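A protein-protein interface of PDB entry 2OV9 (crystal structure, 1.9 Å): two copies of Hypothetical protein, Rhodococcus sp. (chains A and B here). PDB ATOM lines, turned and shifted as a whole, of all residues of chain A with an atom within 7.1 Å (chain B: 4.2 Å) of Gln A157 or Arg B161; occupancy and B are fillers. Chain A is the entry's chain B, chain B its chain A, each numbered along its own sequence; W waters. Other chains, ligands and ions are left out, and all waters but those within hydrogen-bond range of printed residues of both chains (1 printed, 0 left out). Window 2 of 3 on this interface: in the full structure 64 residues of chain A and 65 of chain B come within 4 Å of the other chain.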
ATOM      1  N   ASP A 139     -15.860  11.797  21.036  1.00  0.00           N
ATOM      2  CA  ASP A 139     -16.147  12.106  22.428  1.00  0.00           C
ATOM      3  C   ASP A 139     -15.077  11.481  23.349  1.00  0.00           C
ATOM      4  O   ASP A 139     -14.439  12.178  24.163  1.00  0.00           O
ATOM      5  CB  ASP A 139     -17.545  11.603  22.801  1.00  0.00           C
ATOM      6  CG  ASP A 139     -17.881  11.856  24.252  1.00  0.00           C
ATOM      7  OD1 ASP A 139     -18.249  12.987  24.586  1.00  0.00           O
ATOM      8  OD2 ASP A 139     -17.765  10.933  25.072  1.00  0.00           O
ATOM      9  N   LEU A 142     -11.547  12.977  23.144  1.00  0.00           N
ATOM     10  CA  LEU A 142     -11.463  14.250  23.889  1.00  0.00           C
ATOM     11  C   LEU A 142     -11.254  13.995  25.381  1.00  0.00           C
ATOM     12  O   LEU A 142     -10.481  14.701  26.029  1.00  0.00           O
ATOM     13  CB  LEU A 142     -12.724  15.134  23.696  1.00  0.00           C
ATOM     14  CG  LEU A 142     -13.059  15.585  22.263  1.00  0.00           C
ATOM     15  CD1 LEU A 142     -14.197  16.588  22.299  1.00  0.00           C
ATOM     16  CD2 LEU A 142     -11.830  16.179  21.605  1.00  0.00           C
ATOM     17  N   MET A 154     -16.334  16.650  33.454  1.00  0.00           N
ATOM     18  CA  MET A 154     -17.596  16.066  32.980  1.00  0.00           C
ATOM     19  C   MET A 154     -17.949  16.659  31.631  1.00  0.00           C
ATOM     20  O   MET A 154     -17.791  17.866  31.442  1.00  0.00           O
ATOM     21  CB  MET A 154     -18.732  16.454  33.927  1.00  0.00           C
ATOM     22  CG  MET A 154     -19.032  15.503  35.043  1.00  0.00           C
ATOM     23  SD  MET A 154     -20.729  16.052  35.834  1.00  0.00           S
ATOM     24  CE  MET A 154     -21.956  15.304  34.509  1.00  0.00           C
ATOM     25  N   THR A 155     -18.459  15.852  30.708  1.00  0.00           N
ATOM     26  CA  THR A 155     -18.842  16.386  29.404  1.00  0.00           C
ATOM     27  C   THR A 155     -20.052  17.304  29.591  1.00  0.00           C
ATOM     28  O   THR A 155     -21.004  16.947  30.293  1.00  0.00           O
ATOM     29  CB  THR A 155     -19.137  15.270  28.374  1.00  0.00           C
ATOM     30  OG1 THR A 155     -18.075  14.305  28.386  1.00  0.00           O
ATOM     31  CG2 THR A 155     -19.233  15.841  26.959  1.00  0.00           C
ATOM     32  N   ALA A 156     -19.984  18.493  29.000  1.00  0.00           N
ATOM     33  CA  ALA A 156     -21.103  19.452  29.035  1.00  0.00           C
ATOM     34  C   ALA A 156     -21.789  19.633  27.663  1.00  0.00           C
ATOM     35  O   ALA A 156     -23.023  19.691  27.581  1.00  0.00           O
ATOM     36  CB  ALA A 156     -20.630  20.792  29.570  1.00  0.00           C
ATOM     37  N   GLN A 157     -20.981  19.749  26.606  1.00  0.00           N
ATOM     38  CA  GLN A 157     -21.487  19.942  25.247  1.00  0.00           C
ATOM     39  C   GLN A 157     -20.502  19.395  24.233  1.00  0.00           C
ATOM     40  O   GLN A 157     -19.290  19.534  24.391  1.00  0.00           O
ATOM     41  CB  GLN A 157     -21.758  21.420  24.928  1.00  0.00           C
ATOM     42  CG  GLN A 157     -22.838  21.607  23.855  1.00  0.00           C
ATOM     43  CD  GLN A 157     -22.592  22.777  22.919  1.00  0.00           C
ATOM     44  OE1 GLN A 157     -22.717  23.941  23.302  1.00  0.00           O
ATOM     45  NE2 GLN A 157     -22.276  22.469  21.668  1.00  0.00           N
ATOM     46  N   LEU A 158     -21.026  18.760  23.192  1.00  0.00           N
ATOM     47  CA  LEU A 158     -20.190  18.244  22.124  1.00  0.00           C
ATOM     48  C   LEU A 158     -20.796  18.824  20.857  1.00  0.00           C
ATOM     49  O   LEU A 158     -22.011  18.753  20.670  1.00  0.00           O
ATOM     50  CB  LEU A 158     -20.254  16.712  22.122  1.00  0.00           C
ATOM     51  CG  LEU A 158     -19.219  15.844  21.424  1.00  0.00           C
ATOM     52  CD1 LEU A 158     -17.967  15.710  22.298  1.00  0.00           C
ATOM     53  CD2 LEU A 158     -19.849  14.455  21.108  1.00  0.00           C
ATOM     54  N   SER A 159     -19.973  19.441  20.020  1.00  0.00           N
ATOM     55  CA  SER A 159     -20.424  19.918  18.714  1.00  0.00           C
ATOM     56  C   SER A 159     -19.647  19.223  17.630  1.00  0.00           C
ATOM     57  O   SER A 159     -18.467  19.511  17.463  1.00  0.00           O
ATOM     58  CB  SER A 159     -20.201  21.412  18.590  1.00  0.00           C
ATOM     59  OG  SER A 159     -20.879  22.059  19.652  1.00  0.00           O
ATOM     60  N   THR A 160     -20.308  18.330  16.890  1.00  0.00           N
ATOM     61  CA  THR A 160     -19.628  17.537  15.867  1.00  0.00           C
ATOM     62  C   THR A 160     -20.043  17.984  14.484  1.00  0.00           C
ATOM     63  O   THR A 160     -21.227  18.116  14.201  1.00  0.00           O
ATOM     64  CB  THR A 160     -19.928  16.028  16.064  1.00  0.00           C
ATOM     65  OG1 THR A 160     -19.852  15.723  17.467  1.00  0.00           O
ATOM     66  CG2 THR A 160     -18.931  15.165  15.303  1.00  0.00           C
ATOM     67  N   THR A 188     -11.896  21.333  24.447  1.00  0.00           N
ATOM     68  CA  THR A 188     -11.121  20.301  23.801  1.00  0.00           C
ATOM     69  C   THR A 188     -11.589  20.125  22.359  1.00  0.00           C
ATOM     70  O   THR A 188     -12.791  20.201  22.086  1.00  0.00           O
ATOM     71  CB  THR A 188     -11.286  18.992  24.576  1.00  0.00           C
ATOM     72  OG1 THR A 188     -11.245  19.273  25.981  1.00  0.00           O
ATOM     73  CG2 THR A 188     -10.174  17.978  24.236  1.00  0.00           C
ATOM     74  N   VAL A 203     -14.710  17.860  15.938  1.00  0.00           N
ATOM     75  CA  VAL A 203     -15.491  18.103  17.139  1.00  0.00           C
ATOM     76  C   VAL A 203     -14.856  19.181  18.001  1.00  0.00           C
ATOM     77  O   VAL A 203     -13.629  19.369  17.978  1.00  0.00           O
ATOM     78  CB  VAL A 203     -15.670  16.804  17.968  1.00  0.00           C
ATOM     79  CG1 VAL A 203     -14.321  16.298  18.499  1.00  0.00           C
ATOM     80  CG2 VAL A 203     -16.682  17.026  19.127  1.00  0.00           C
ATOM     81  N   GLU A 204     -15.728  19.932  18.670  1.00  0.00           N
ATOM     82  CA  GLU A 204     -15.380  20.815  19.787  1.00  0.00           C
ATOM     83  C   GLU A 204     -16.206  20.377  21.001  1.00  0.00           C
ATOM     84  O   GLU A 204     -17.452  20.362  20.917  1.00  0.00           O
ATOM     85  CB  GLU A 204     -15.745  22.272  19.467  1.00  0.00           C
ATOM     86  CG  GLU A 204     -14.808  23.024  18.521  1.00  0.00           C
ATOM     87  CD  GLU A 204     -15.282  24.447  18.192  1.00  0.00           C
ATOM     88  OE1 GLU A 204     -16.081  25.036  18.967  1.00  0.00           O
ATOM     89  OE2 GLU A 204     -14.850  24.985  17.145  1.00  0.00           O
ATOM     90  N   GLY A 205     -15.544  20.051  22.111  1.00  0.00           N
ATOM     91  CA  GLY A 205     -16.253  19.705  23.359  1.00  0.00           C
ATOM     92  C   GLY A 205     -15.932  20.661  24.490  1.00  0.00           C
ATOM     93  O   GLY A 205     -14.826  21.213  24.575  1.00  0.00           O
ATOM     94  N   LEU A 206     -16.920  20.855  25.352  1.00  0.00           N
ATOM     95  CA  LEU A 206     -16.791  21.687  26.530  1.00  0.00           C
ATOM     96  C   LEU A 206     -16.941  20.780  27.728  1.00  0.00           C
ATOM     97  O   LEU A 206     -17.829  19.914  27.764  1.00  0.00           O
ATOM     98  CB  LEU A 206     -17.860  22.783  26.544  1.00  0.00           C
ATOM     99  CG  LEU A 206     -17.871  23.766  25.364  1.00  0.00           C
ATOM    100  CD1 LEU A 206     -19.095  24.685  25.427  1.00  0.00           C
ATOM    101  CD2 LEU A 206     -16.574  24.599  25.302  1.00  0.00           C
ATOM    102  N   PHE A 207     -16.059  20.967  28.704  1.00  0.00           N
ATOM    103  CA  PHE A 207     -16.014  20.102  29.869  1.00  0.00           C
ATOM    104  C   PHE A 207     -15.980  20.959  31.129  1.00  0.00           C
ATOM    105  O   PHE A 207     -15.682  22.154  31.071  1.00  0.00           O
ATOM    106  CB  PHE A 207     -14.799  19.168  29.799  1.00  0.00           C
ATOM    107  CG  PHE A 207     -14.816  18.226  28.621  1.00  0.00           C
ATOM    108  CD1 PHE A 207     -15.269  16.918  28.770  1.00  0.00           C
ATOM    109  CD2 PHE A 207     -14.378  18.640  27.371  1.00  0.00           C
ATOM    110  CE1 PHE A 207     -15.292  16.039  27.690  1.00  0.00           C
ATOM    111  CE2 PHE A 207     -14.395  17.766  26.262  1.00  0.00           C
ATOM    112  CZ  PHE A 207     -14.842  16.467  26.421  1.00  0.00           C
ATOM    113  N   VAL A 208     -16.301  20.346  32.264  1.00  0.00           N
ATOM    114  CA  VAL A 208     -16.320  21.059  33.539  1.00  0.00           C
ATOM    115  C   VAL A 208     -15.580  20.257  34.613  1.00  0.00           C
ATOM    116  O   VAL A 208     -16.038  19.179  34.999  1.00  0.00           O
ATOM    117  CB  VAL A 208     -17.768  21.352  34.007  1.00  0.00           C
ATOM    118  CG1 VAL A 208     -17.790  22.348  35.188  1.00  0.00           C
ATOM    119  CG2 VAL A 208     -18.617  21.879  32.851  1.00  0.00           C
ATOM    120  N   SER B 159     -25.220  18.991  17.661  1.00  0.00           N
ATOM    121  CA  SER B 159     -24.825  19.715  18.869  1.00  0.00           C
ATOM    122  C   SER B 159     -25.520  19.054  20.052  1.00  0.00           C
ATOM    123  O   SER B 159     -26.751  19.098  20.161  1.00  0.00           O
ATOM    124  CB  SER B 159     -25.218  21.200  18.785  1.00  0.00           C
ATOM    125  OG  SER B 159     -24.499  21.897  17.769  1.00  0.00           O
ATOM    126  N   THR B 160     -24.732  18.426  20.923  1.00  0.00           N
ATOM    127  CA  THR B 160     -25.245  17.537  21.970  1.00  0.00           C
ATOM    128  C   THR B 160     -24.957  18.190  23.301  1.00  0.00           C
ATOM    129  O   THR B 160     -23.821  18.564  23.562  1.00  0.00           O
ATOM    130  CB  THR B 160     -24.543  16.135  21.877  1.00  0.00           C
ATOM    131  OG1 THR B 160     -24.801  15.551  20.591  1.00  0.00           O
ATOM    132  CG2 THR B 160     -25.042  15.187  22.952  1.00  0.00           C
ATOM    133  N   ARG B 161     -25.992  18.360  24.125  1.00  0.00           N
ATOM    134  CA  ARG B 161     -25.875  19.052  25.407  1.00  0.00           C
ATOM    135  C   ARG B 161     -26.167  18.056  26.496  1.00  0.00           C
ATOM    136  O   ARG B 161     -27.145  17.323  26.409  1.00  0.00           O
ATOM    137  CB  ARG B 161     -26.886  20.207  25.507  1.00  0.00           C
ATOM    138  CG  ARG B 161     -26.995  21.003  24.229  1.00  0.00           C
ATOM    139  CD  ARG B 161     -27.434  22.449  24.444  1.00  0.00           C
ATOM    140  NE  ARG B 161     -26.676  23.340  23.563  1.00  0.00           N
ATOM    141  CZ  ARG B 161     -26.016  24.422  23.970  1.00  0.00           C
ATOM    142  NH1 ARG B 161     -26.046  24.779  25.250  1.00  0.00           N
ATOM    143  NH2 ARG B 161     -25.348  25.166  23.087  1.00  0.00           N
ATOM    144  N   TYR B 162     -25.322  18.029  27.515  1.00  0.00           N
ATOM    145  CA  TYR B 162     -25.461  17.054  28.591  1.00  0.00           C
ATOM    146  C   TYR B 162     -25.988  17.754  29.833  1.00  0.00           C
ATOM    147  O   TYR B 162     -25.294  18.578  30.423  1.00  0.00           O
ATOM    148  CB  TYR B 162     -24.117  16.370  28.864  1.00  0.00           C
ATOM    149  CG  TYR B 162     -23.643  15.572  27.664  1.00  0.00           C
ATOM    150  CD1 TYR B 162     -23.994  14.225  27.521  1.00  0.00           C
ATOM    151  CD2 TYR B 162     -22.898  16.176  26.644  1.00  0.00           C
ATOM    152  CE1 TYR B 162     -23.606  13.501  26.382  1.00  0.00           C
ATOM    153  CE2 TYR B 162     -22.489  15.459  25.529  1.00  0.00           C
ATOM    154  CZ  TYR B 162     -22.853  14.125  25.405  1.00  0.00           C
ATOM    155  OH  TYR B 162     -22.457  13.409  24.299  1.00  0.00           O
ATOM    156  N   HIS B 163     -27.214  17.426  30.220  1.00  0.00           N
ATOM    157  CA  HIS B 163     -27.881  18.146  31.308  1.00  0.00           C
ATOM    158  C   HIS B 163     -27.712  17.440  32.640  1.00  0.00           C
ATOM    159  O   HIS B 163     -27.439  18.084  33.649  1.00  0.00           O
ATOM    160  CB  HIS B 163     -29.378  18.340  31.023  1.00  0.00           C
ATOM    161  CG  HIS B 163     -29.668  18.870  29.655  1.00  0.00           C
ATOM    162  ND1 HIS B 163     -30.242  20.106  29.444  1.00  0.00           N
ATOM    163  CD2 HIS B 163     -29.478  18.326  28.431  1.00  0.00           C
ATOM    164  CE1 HIS B 163     -30.376  20.304  28.143  1.00  0.00           C
ATOM    165  NE2 HIS B 163     -29.923  19.239  27.508  1.00  0.00           N
ATOM    166  N   VAL B 201     -29.846  14.158  28.200  1.00  0.00           N
ATOM    167  CA  VAL B 201     -29.076  14.643  27.064  1.00  0.00           C
ATOM    168  C   VAL B 201     -30.040  15.143  26.002  1.00  0.00           C
ATOM    169  O   VAL B 201     -31.095  14.540  25.812  1.00  0.00           O
ATOM    170  CB  VAL B 201     -28.218  13.512  26.438  1.00  0.00           C
ATOM    171  CG1 VAL B 201     -27.259  14.084  25.412  1.00  0.00           C
ATOM    172  CG2 VAL B 201     -27.443  12.764  27.517  1.00  0.00           C
ATOM    173  N   SER B 202     -29.709  16.256  25.337  1.00  0.00           N
ATOM    174  CA  SER B 202     -30.508  16.747  24.214  1.00  0.00           C
ATOM    175  C   SER B 202     -29.610  17.050  23.035  1.00  0.00           C
ATOM    176  O   SER B 202     -28.387  17.184  23.159  1.00  0.00           O
ATOM    177  CB  SER B 202     -31.356  17.968  24.584  1.00  0.00           C
ATOM    178  OG  SER B 202     -30.524  19.070  24.866  1.00  0.00           O
HETATM  179  O   HOH W   1     -22.271  16.023  19.066  1.00  0.00           O
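N of Thr B160 sits at hydrogen-bond distance from O of Leu A158.
The side-chain amide oxygen (OE1) of Gln A157 sits at hydrogen-bond distance from the guanidinium group (NH2) of Arg B161 (2.9 Å).
The backbone NH (N) of Tyr B162 is in hydrogen-bond range of the backbone carbonyl oxygen (O) of Ala A156, at 2.8 Å.
N of Arg B161 lies within hydrogen-bond range of O of Ser B202 (2.8 Å).
O of Leu A206 is in hydrogen-bond range of N of Ala A156 (2.9 Å).
The side-chain hydroxyl (OG) of Ser A159 lies within hydrogen-bond range of the side-chain amide nitrogen (NE2) of Gln A157 (2.5 Å).
The backbone carbonyl oxygen of Gln A157 is in hydrogen-bond range of the backbone NH of Leu A206 (2.9 Å).
Among the printed residues, merely in contact across the chains: Gln A157 with Thr B160, Thr A155 with Tyr B162, Leu A158 with Ser B159 and Ala A156 with Arg B161.
Of the printed residues of chain B, Gln A157 touches Thr B160 and Arg B161.
Of the printed residues of chain B, Leu A158 touches Ser B159 and Thr B160.
Printed residues of chain A within 4 Å of Thr B160: Gln A157 (3.2 Å) and Leu A158 (2.8 Å).
Printed residues of chain A within 4 Å of Arg B161: Ala A156 and Gln A157.
The nearest printed residue of chain B that does not touch Leu A158 is Tyr B162 (4.3 Å).
Of the 7 printed residues of chain B, 4 touch a printed residue of chain A.
Printed residues of chain A that touch a printed residue of chain B: Thr A155, Ala A156, Gln A157 and Leu A158.
Among the printed residues, 7 pairs touch across the chains.
Positions printed for both chains: 159 and 160.
Of the 7 pairs that touch across the chains among the printed residues, none has its exchanged pair printed and touching as well.
Water W1 lies within hydrogen-bond range of OG1 of Thr A160 (2.9 Å), OG1 of Thr B160 (3.0 Å) and O of Leu A158 (3.2 Å).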
